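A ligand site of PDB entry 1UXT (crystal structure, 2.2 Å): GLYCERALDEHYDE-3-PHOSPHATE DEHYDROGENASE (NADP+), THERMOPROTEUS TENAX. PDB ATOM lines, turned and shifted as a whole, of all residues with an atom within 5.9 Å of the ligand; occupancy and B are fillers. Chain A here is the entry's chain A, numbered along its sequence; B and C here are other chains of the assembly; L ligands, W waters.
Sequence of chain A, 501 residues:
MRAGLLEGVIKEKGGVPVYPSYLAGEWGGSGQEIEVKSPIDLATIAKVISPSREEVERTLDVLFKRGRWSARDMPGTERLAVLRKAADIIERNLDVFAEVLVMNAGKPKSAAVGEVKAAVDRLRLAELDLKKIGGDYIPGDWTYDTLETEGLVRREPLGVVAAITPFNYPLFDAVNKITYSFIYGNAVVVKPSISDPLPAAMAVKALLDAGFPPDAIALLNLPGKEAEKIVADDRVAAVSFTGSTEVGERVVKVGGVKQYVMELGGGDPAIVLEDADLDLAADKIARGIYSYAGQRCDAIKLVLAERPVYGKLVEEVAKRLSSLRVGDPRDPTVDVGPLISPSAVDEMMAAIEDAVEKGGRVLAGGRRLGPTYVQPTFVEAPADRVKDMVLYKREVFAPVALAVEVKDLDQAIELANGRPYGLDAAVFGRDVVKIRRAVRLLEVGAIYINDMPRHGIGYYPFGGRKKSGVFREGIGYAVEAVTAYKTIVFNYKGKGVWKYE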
ATOM      1  N   ALA A  71      14.087 -10.126   5.546  1.00  0.00           N
ATOM      2  CA  ALA A  71      13.085 -11.170   5.358  1.00  0.00           C
ATOM      3  C   ALA A  71      13.795 -12.444   4.934  1.00  0.00           C
ATOM      4  O   ALA A  71      13.624 -13.503   5.528  1.00  0.00           O
ATOM      5  CB  ALA A  71      12.084 -10.750   4.286  1.00  0.00           C
ATOM      6  N   ARG A  72      14.618 -12.345   3.910  1.00  0.00           N
ATOM      7  CA  ARG A  72      15.320 -13.515   3.378  1.00  0.00           C
ATOM      8  C   ARG A  72      16.318 -14.101   4.375  1.00  0.00           C
ATOM      9  O   ARG A  72      16.442 -15.324   4.486  1.00  0.00           O
ATOM     10  CB  ARG A  72      16.042 -13.111   2.093  1.00  0.00           C
ATOM     11  CG  ARG A  72      16.689 -14.258   1.361  1.00  0.00           C
ATOM     12  CD  ARG A  72      17.273 -13.796   0.028  1.00  0.00           C
ATOM     13  NE  ARG A  72      17.861 -14.896  -0.715  1.00  0.00           N
ATOM     14  CZ  ARG A  72      18.605 -14.768  -1.814  1.00  0.00           C
ATOM     15  NH1 ARG A  72      18.840 -13.559  -2.311  1.00  0.00           N
ATOM     16  NH2 ARG A  72      19.151 -15.834  -2.407  1.00  0.00           N
ATOM     17  N   ASP A  73      16.990 -13.239   5.123  1.00  0.00           N
ATOM     18  CA  ASP A  73      17.968 -13.746   6.069  1.00  0.00           C
ATOM     19  C   ASP A  73      17.416 -14.203   7.392  1.00  0.00           C
ATOM     20  O   ASP A  73      18.161 -14.584   8.288  1.00  0.00           O
ATOM     21  CB  ASP A  73      19.139 -12.762   6.224  1.00  0.00           C
ATOM     22  CG  ASP A  73      20.041 -12.728   4.956  1.00  0.00           C
ATOM     23  OD1 ASP A  73      19.989 -13.703   4.146  1.00  0.00           O
ATOM     24  OD2 ASP A  73      20.800 -11.754   4.757  1.00  0.00           O
ATOM     25  N   MET A  74      16.087 -14.161   7.513  1.00  0.00           N
ATOM     26  CA  MET A  74      15.433 -14.713   8.695  1.00  0.00           C
ATOM     27  C   MET A  74      15.085 -16.144   8.209  1.00  0.00           C
ATOM     28  O   MET A  74      14.273 -16.331   7.307  1.00  0.00           O
ATOM     29  CB  MET A  74      14.126 -13.977   9.036  1.00  0.00           C
ATOM     30  CG  MET A  74      13.311 -14.736  10.077  1.00  0.00           C
ATOM     31  SD  MET A  74      11.868 -13.830  10.740  1.00  0.00           S
ATOM     32  CE  MET A  74      12.743 -12.503  11.858  1.00  0.00           C
ATOM     33  N   PRO A  75      15.686 -17.175   8.797  1.00  0.00           N
ATOM     34  CA  PRO A  75      15.351 -18.510   8.314  1.00  0.00           C
ATOM     35  C   PRO A  75      13.861 -18.851   8.407  1.00  0.00           C
ATOM     36  O   PRO A  75      13.138 -18.362   9.281  1.00  0.00           O
ATOM     37  CB  PRO A  75      16.217 -19.406   9.160  1.00  0.00           C
ATOM     38  CG  PRO A  75      16.280 -18.660  10.472  1.00  0.00           C
ATOM     39  CD  PRO A  75      16.489 -17.233  10.043  1.00  0.00           C
ATOM     40  N   GLY A  76      13.413 -19.738   7.509  1.00  0.00           N
ATOM     41  CA  GLY A  76      12.015 -20.130   7.501  1.00  0.00           C
ATOM     42  C   GLY A  76      11.487 -20.624   8.843  1.00  0.00           C
ATOM     43  O   GLY A  76      10.331 -20.379   9.207  1.00  0.00           O
ATOM     44  N   ARG A  79      10.473 -17.560  10.474  1.00  0.00           N
ATOM     45  CA  ARG A  79       9.373 -16.858   9.856  1.00  0.00           C
ATOM     46  C   ARG A  79       8.074 -17.500  10.327  1.00  0.00           C
ATOM     47  O   ARG A  79       7.093 -16.822  10.589  1.00  0.00           O
ATOM     48  CB  ARG A  79       9.424 -16.940   8.327  1.00  0.00           C
ATOM     49  CG  ARG A  79      10.644 -16.333   7.699  1.00  0.00           C
ATOM     50  CD  ARG A  79      10.484 -16.228   6.183  1.00  0.00           C
ATOM     51  NE  ARG A  79      11.809 -16.045   5.596  1.00  0.00           N
ATOM     52  CZ  ARG A  79      12.330 -16.842   4.669  1.00  0.00           C
ATOM     53  NH1 ARG A  79      11.650 -17.863   4.181  1.00  0.00           N
ATOM     54  NH2 ARG A  79      13.589 -16.645   4.295  1.00  0.00           N
ATOM     55  N   ILE A 133       7.522 -25.730  -1.966  1.00  0.00           N
ATOM     56  CA  ILE A 133       8.767 -24.959  -1.852  1.00  0.00           C
ATOM     57  C   ILE A 133      10.043 -25.682  -2.312  1.00  0.00           C
ATOM     58  O   ILE A 133      11.065 -25.041  -2.572  1.00  0.00           O
ATOM     59  CB  ILE A 133       9.040 -24.475  -0.419  1.00  0.00           C
ATOM     60  CG1 ILE A 133       9.916 -23.221  -0.466  1.00  0.00           C
ATOM     61  CG2 ILE A 133       9.803 -25.547   0.363  1.00  0.00           C
ATOM     62  CD1 ILE A 133      10.263 -22.645   0.883  1.00  0.00           C
ATOM     63  N   ARG A 154      15.778 -24.194  -8.147  1.00  0.00           N
ATOM     64  CA  ARG A 154      15.209 -23.892  -6.849  1.00  0.00           C
ATOM     65  C   ARG A 154      14.519 -22.550  -6.841  1.00  0.00           C
ATOM     66  O   ARG A 154      14.792 -21.682  -7.682  1.00  0.00           O
ATOM     67  CB  ARG A 154      16.292 -23.994  -5.761  1.00  0.00           C
ATOM     68  CG  ARG A 154      17.090 -22.757  -5.517  1.00  0.00           C
ATOM     69  CD  ARG A 154      18.380 -23.043  -4.727  1.00  0.00           C
ATOM     70  NE  ARG A 154      18.254 -23.520  -3.340  1.00  0.00           N
ATOM     71  CZ  ARG A 154      18.049 -22.729  -2.289  1.00  0.00           C
ATOM     72  NH1 ARG A 154      17.948 -21.429  -2.467  1.00  0.00           N
ATOM     73  NH2 ARG A 154      18.045 -23.226  -1.058  1.00  0.00           N
ATOM     74  N   ARG A 155      13.582 -22.374  -5.906  1.00  0.00           N
ATOM     75  CA  ARG A 155      12.858 -21.111  -5.819  1.00  0.00           C
ATOM     76  C   ARG A 155      13.615 -20.090  -4.994  1.00  0.00           C
ATOM     77  O   ARG A 155      14.317 -20.430  -4.047  1.00  0.00           O
ATOM     78  CB  ARG A 155      11.475 -21.356  -5.256  1.00  0.00           C
ATOM     79  CG  ARG A 155      10.987 -22.732  -5.569  1.00  0.00           C
ATOM     80  CD  ARG A 155       9.508 -22.865  -5.667  1.00  0.00           C
ATOM     81  NE  ARG A 155       8.977 -22.251  -6.876  1.00  0.00           N
ATOM     82  CZ  ARG A 155       7.981 -22.770  -7.577  1.00  0.00           C
ATOM     83  NH1 ARG A 155       7.427 -23.921  -7.171  1.00  0.00           N
ATOM     84  NH2 ARG A 155       7.525 -22.145  -8.650  1.00  0.00           N
ATOM     85  N   GLU A 156      13.452 -18.840  -5.368  1.00  0.00           N
ATOM     86  CA  GLU A 156      14.110 -17.755  -4.680  1.00  0.00           C
ATOM     87  C   GLU A 156      13.121 -16.597  -4.524  1.00  0.00           C
ATOM     88  O   GLU A 156      12.278 -16.368  -5.386  1.00  0.00           O
ATOM     89  CB  GLU A 156      15.305 -17.285  -5.515  1.00  0.00           C
ATOM     90  CG  GLU A 156      16.481 -16.867  -4.687  1.00  0.00           C
ATOM     91  CD  GLU A 156      17.724 -16.497  -5.516  1.00  0.00           C
ATOM     92  OE1 GLU A 156      17.658 -15.501  -6.269  1.00  0.00           O
ATOM     93  OE2 GLU A 156      18.754 -17.212  -5.392  1.00  0.00           O
ATOM     94  N   PRO A 157      13.184 -15.859  -3.389  1.00  0.00           N
ATOM     95  CA  PRO A 157      12.224 -14.765  -3.289  1.00  0.00           C
ATOM     96  C   PRO A 157      12.502 -13.731  -4.382  1.00  0.00           C
ATOM     97  O   PRO A 157      13.646 -13.557  -4.782  1.00  0.00           O
ATOM     98  CB  PRO A 157      12.471 -14.187  -1.879  1.00  0.00           C
ATOM     99  CG  PRO A 157      13.903 -14.653  -1.539  1.00  0.00           C
ATOM    100  CD  PRO A 157      13.938 -16.047  -2.133  1.00  0.00           C
ATOM    101  N   ILE A 183       6.511 -15.801   3.796  1.00  0.00           N
ATOM    102  CA  ILE A 183       6.948 -17.155   3.988  1.00  0.00           C
ATOM    103  C   ILE A 183       8.053 -17.602   2.997  1.00  0.00           C
ATOM    104  O   ILE A 183       8.911 -18.399   3.351  1.00  0.00           O
ATOM    105  CB  ILE A 183       5.725 -18.107   3.982  1.00  0.00           C
ATOM    106  CG1 ILE A 183       6.096 -19.432   4.649  1.00  0.00           C
ATOM    107  CG2 ILE A 183       5.204 -18.329   2.588  1.00  0.00           C
ATOM    108  CD1 ILE A 183       6.566 -19.243   6.096  1.00  0.00           C
ATOM    109  N   TYR A 184       8.046 -17.054   1.782  1.00  0.00           N
ATOM    110  CA  TYR A 184       9.064 -17.416   0.790  1.00  0.00           C
ATOM    111  C   TYR A 184      10.301 -16.495   0.822  1.00  0.00           C
ATOM    112  O   TYR A 184      11.181 -16.637  -0.016  1.00  0.00           O
ATOM    113  CB  TYR A 184       8.441 -17.450  -0.635  1.00  0.00           C
ATOM    114  CG  TYR A 184       7.408 -18.537  -0.753  1.00  0.00           C
ATOM    115  CD1 TYR A 184       7.744 -19.875  -0.502  1.00  0.00           C
ATOM    116  CD2 TYR A 184       6.070 -18.234  -1.014  1.00  0.00           C
ATOM    117  CE1 TYR A 184       6.764 -20.877  -0.498  1.00  0.00           C
ATOM    118  CE2 TYR A 184       5.096 -19.213  -1.004  1.00  0.00           C
ATOM    119  CZ  TYR A 184       5.437 -20.535  -0.739  1.00  0.00           C
ATOM    120  OH  TYR A 184       4.454 -21.528  -0.715  1.00  0.00           O
ATOM    121  N   GLY A 185      10.346 -15.560   1.770  1.00  0.00           N
ATOM    122  CA  GLY A 185      11.495 -14.680   1.929  1.00  0.00           C
ATOM    123  C   GLY A 185      11.457 -13.287   1.367  1.00  0.00           C
ATOM    124  O   GLY A 185      12.507 -12.644   1.238  1.00  0.00           O
ATOM    125  N   PRO B 139      15.570 -27.437   0.795  1.00  0.00           N
ATOM    126  CA  PRO B 139      16.263 -26.342   1.515  1.00  0.00           C
ATOM    127  C   PRO B 139      16.338 -26.701   3.017  1.00  0.00           C
ATOM    128  O   PRO B 139      15.452 -27.396   3.539  1.00  0.00           O
ATOM    129  CB  PRO B 139      15.403 -25.129   1.226  1.00  0.00           C
ATOM    130  CG  PRO B 139      13.999 -25.731   1.054  1.00  0.00           C
ATOM    131  CD  PRO B 139      14.236 -27.031   0.306  1.00  0.00           C
ATOM    132  N   GLY B 140      17.396 -26.288   3.704  1.00  0.00           N
ATOM    133  CA  GLY B 140      17.517 -26.669   5.107  1.00  0.00           C
ATOM    134  C   GLY B 140      17.072 -25.714   6.203  1.00  0.00           C
ATOM    135  O   GLY B 140      17.102 -26.081   7.373  1.00  0.00           O
ATOM    136  N   ASP B 141      16.631 -24.512   5.843  1.00  0.00           N
ATOM    137  CA  ASP B 141      16.260 -23.522   6.860  1.00  0.00           C
ATOM    138  C   ASP B 141      14.865 -23.640   7.505  1.00  0.00           C
ATOM    139  O   ASP B 141      14.420 -22.710   8.161  1.00  0.00           O
ATOM    140  CB  ASP B 141      16.431 -22.093   6.291  1.00  0.00           C
ATOM    141  CG  ASP B 141      15.557 -21.823   5.059  1.00  0.00           C
ATOM    142  OD1 ASP B 141      15.762 -22.513   4.016  1.00  0.00           O
ATOM    143  OD2 ASP B 141      14.679 -20.928   5.117  1.00  0.00           O
ATOM    144  N   TRP B 142      14.213 -24.790   7.379  1.00  0.00           N
ATOM    145  CA  TRP B 142      12.880 -24.925   7.954  1.00  0.00           C
ATOM    146  C   TRP B 142      12.916 -25.592   9.302  1.00  0.00           C
ATOM    147  O   TRP B 142      11.885 -25.784   9.930  1.00  0.00           O
ATOM    148  CB  TRP B 142      11.929 -25.635   6.957  1.00  0.00           C
ATOM    149  CG  TRP B 142      11.712 -24.695   5.784  1.00  0.00           C
ATOM    150  CD1 TRP B 142      12.436 -24.647   4.631  1.00  0.00           C
ATOM    151  CD2 TRP B 142      10.905 -23.497   5.795  1.00  0.00           C
ATOM    152  NE1 TRP B 142      12.161 -23.490   3.921  1.00  0.00           N
ATOM    153  CE2 TRP B 142      11.219 -22.767   4.612  1.00  0.00           C
ATOM    154  CE3 TRP B 142       9.947 -22.961   6.683  1.00  0.00           C
ATOM    155  CZ2 TRP B 142      10.625 -21.544   4.304  1.00  0.00           C
ATOM    156  CZ3 TRP B 142       9.362 -21.730   6.367  1.00  0.00           C
ATOM    157  CH2 TRP B 142       9.703 -21.038   5.190  1.00  0.00           C
ATOM    158  N   TRP B 498      24.852 -18.468   3.854  1.00  0.00           N
ATOM    159  CA  TRP B 498      23.685 -17.795   4.437  1.00  0.00           C
ATOM    160  C   TRP B 498      24.159 -16.942   5.633  1.00  0.00           C
ATOM    161  O   TRP B 498      25.233 -17.194   6.188  1.00  0.00           O
ATOM    162  CB  TRP B 498      22.682 -18.837   4.933  1.00  0.00           C
ATOM    163  CG  TRP B 498      21.992 -19.561   3.818  1.00  0.00           C
ATOM    164  CD1 TRP B 498      20.963 -19.098   3.047  1.00  0.00           C
ATOM    165  CD2 TRP B 498      22.337 -20.851   3.296  1.00  0.00           C
ATOM    166  NE1 TRP B 498      20.631 -20.026   2.094  1.00  0.00           N
ATOM    167  CE2 TRP B 498      21.453 -21.109   2.219  1.00  0.00           C
ATOM    168  CE3 TRP B 498      23.288 -21.813   3.635  1.00  0.00           C
ATOM    169  CZ2 TRP B 498      21.516 -22.296   1.472  1.00  0.00           C
ATOM    170  CZ3 TRP B 498      23.347 -22.985   2.901  1.00  0.00           C
ATOM    171  CH2 TRP B 498      22.459 -23.222   1.829  1.00  0.00           C
ATOM    172  N   GLU B 501      20.319 -18.230   8.214  1.00  0.00           N
ATOM    173  CA  GLU B 501      19.103 -18.578   7.448  1.00  0.00           C
ATOM    174  C   GLU B 501      19.302 -19.666   6.396  1.00  0.00           C
ATOM    175  O   GLU B 501      18.629 -19.647   5.346  1.00  0.00           O
ATOM    176  CB  GLU B 501      18.563 -17.335   6.773  1.00  0.00           C
ATOM    177  OXT GLU B 501      20.022 -20.396   6.971  1.00  0.00           O
ATOM    178  N   ARG C 436      28.961 -22.442  -3.926  1.00  0.00           N
ATOM    179  CA  ARG C 436      27.642 -22.295  -3.297  1.00  0.00           C
ATOM    180  C   ARG C 436      27.318 -20.846  -2.969  1.00  0.00           C
ATOM    181  O   ARG C 436      26.182 -20.414  -3.144  1.00  0.00           O
ATOM    182  CB  ARG C 436      27.534 -23.133  -2.033  1.00  0.00           C
ATOM    183  CG  ARG C 436      26.091 -23.146  -1.493  1.00  0.00           C
ATOM    184  CD  ARG C 436      25.143 -23.801  -2.522  1.00  0.00           C
ATOM    185  NE  ARG C 436      23.739 -23.777  -2.137  1.00  0.00           N
ATOM    186  CZ  ARG C 436      22.929 -22.725  -2.224  1.00  0.00           C
ATOM    187  NH1 ARG C 436      23.383 -21.566  -2.670  1.00  0.00           N
ATOM    188  NH2 ARG C 436      21.641 -22.839  -1.923  1.00  0.00           N
ATOM    189  N   ARG C 440      24.133 -18.583  -4.511  1.00  0.00           N
ATOM    190  CA  ARG C 440      23.123 -17.872  -3.735  1.00  0.00           C
ATOM    191  C   ARG C 440      23.021 -16.394  -4.025  1.00  0.00           C
ATOM    192  O   ARG C 440      21.910 -15.878  -4.196  1.00  0.00           O
ATOM    193  CB  ARG C 440      23.359 -18.057  -2.225  1.00  0.00           C
ATOM    194  CG  ARG C 440      22.380 -17.219  -1.382  1.00  0.00           C
ATOM    195  CD  ARG C 440      22.260 -17.711   0.071  1.00  0.00           C
ATOM    196  NE  ARG C 440      21.213 -16.964   0.748  1.00  0.00           N
ATOM    197  CZ  ARG C 440      21.383 -15.830   1.412  1.00  0.00           C
ATOM    198  NH1 ARG C 440      22.597 -15.287   1.545  1.00  0.00           N
ATOM    199  NH2 ARG C 440      20.317 -15.199   1.888  1.00  0.00           N
HETATM  200  C1  LIG L   1      15.035 -18.896  -0.108  1.00  0.00           C
HETATM  201  C2  LIG L   1      14.248 -18.734   1.188  1.00  0.00           C
HETATM  202  C3  LIG L   1      14.348 -19.986   2.076  1.00  0.00           C
HETATM  203  C4  LIG L   1      13.771 -21.118   1.187  1.00  0.00           C
HETATM  204  C5  LIG L   1      14.640 -21.368  -0.044  1.00  0.00           C
HETATM  205  C6  LIG L   1      14.035 -22.335  -1.055  1.00  0.00           C
HETATM  206  O1  LIG L   1      16.352 -18.473   0.337  1.00  0.00           O
HETATM  207  O2  LIG L   1      14.775 -17.569   1.898  1.00  0.00           O
HETATM  208  O3  LIG L   1      13.531 -19.710   3.247  1.00  0.00           O
HETATM  209  O4  LIG L   1      13.852 -22.247   2.036  1.00  0.00           O
HETATM  210  O5  LIG L   1      15.131 -20.230  -0.706  1.00  0.00           O
HETATM  211  O6  LIG L   1      14.907 -22.484  -2.199  1.00  0.00           O
HETATM  212  P1  LIG L   1      17.863 -18.574  -0.252  1.00  0.00           P
HETATM  213  O7  LIG L   1      18.571 -19.937  -0.199  1.00  0.00           O
HETATM  214  O8  LIG L   1      17.927 -17.847  -1.777  1.00  0.00           O
HETATM  215  O9  LIG L   1      18.737 -17.637   0.785  1.00  0.00           O
HETATM  216  O   HOH W   1      17.479 -17.953   3.236  1.00  0.00           O
HETATM  217  O   HOH W   2      13.420 -24.378  -3.699  1.00  0.00           O
HETATM  218  O   HOH W   3      20.656 -20.117  -2.342  1.00  0.00           O
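NH2 of Arg 72 lies within hydrogen-bond range of O of Arg 440 of chain C. The backbone carbonyl oxygen of Ile 183 lies within hydrogen-bond range of the guanidinium group of Arg 79. N of Arg 72 lies within hydrogen-bond range of O of Gly 185, at 3.4 Å. O of Arg 72 lies within hydrogen-bond range of NH2 of Arg 79 (3.1 Å). N of Gly 76 lies within hydrogen-bond range of OD2 of Asp 141 of chain B (3.0 Å). NE of Arg 79 is in hydrogen-bond range of O of Ala 71, at 3.1 Å. OD1 of Asp 73 lies within salt-bridge range of NH2 of Arg 440 of chain C. The guanidinium group (NE) of Arg 79 sits at hydrogen-bond distance from the backbone carbonyl oxygen (O) of Met 74, at 3.0 Å.
An oxygen (O7) of the ligand lies within salt-bridge range of the guanidinium group of Arg 154, 2.8 Å away. The backbone carbonyl oxygen (O) of Arg 155 lies within hydrogen-bond range of an oxygen (O6) of the ligand (2.8 Å). NE of Arg 440 of chain C lies within salt-bridge range of O9 of the ligand (2.6 Å). The side-chain carboxylate of Asp 141 of chain B sits at hydrogen-bond distance from an oxygen (O3) of the ligand (2.5 Å). NH1 of Arg 79 lies within hydrogen-bond range of O3 of the ligand (2.8 Å). An oxygen (O4) of the ligand sits at hydrogen-bond distance from the indole nitrogen of Trp 142 of chain B (2.8 Å). NH2 of Arg 72 is in salt-bridge range of O8 of the ligand, at 2.4 Å. An oxygen (O7) of the ligand is in hydrogen-bond range of the indole nitrogen of Trp 498 of chain B (3.1 Å).
Residues that only touch the ligand: Ile 133 (3.8 Å), Glu 156 (3.4 Å), Pro 157 (3.7 Å), Tyr 184 (3.9 Å) and Pro 139 of chain B (3.4 Å). Hydrophobic or aromatic side chains within 4 Å of the ligand: Ile 133, Pro 157, Pro 139 of chain B, Trp 142 of chain B and Trp 498 of chain B. Within 4 Å of the ligand: Arg 72, Arg 79, Ile 133, Arg 154, Arg 155, Glu 156, Pro 157, Tyr 184, Pro 139 of chain B, Asp 141 of chain B, Trp 142 of chain B, Trp 498 of chain B and Arg 440 of chain C. The nearest printed residue that does not touch the ligand is Gly 76 (4.3 Å).
Water W1 lies within hydrogen-bond range of O9 of the ligand (2.8 Å), O of Glu 501 of chain B (2.9 Å) and O of Arg 72 (3.1 Å). Water W2 lies within hydrogen-bond range of O of Ile 133 (2.7 Å), O6 of the ligand (2.8 Å) and N of Arg 155 (3.0 Å). Water W3 lies within hydrogen-bond range of NH2 of Arg 436 of chain C (2.9 Å), O7 of the ligand (3.0 Å) and NH1 of Arg 154 (3.0 Å).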
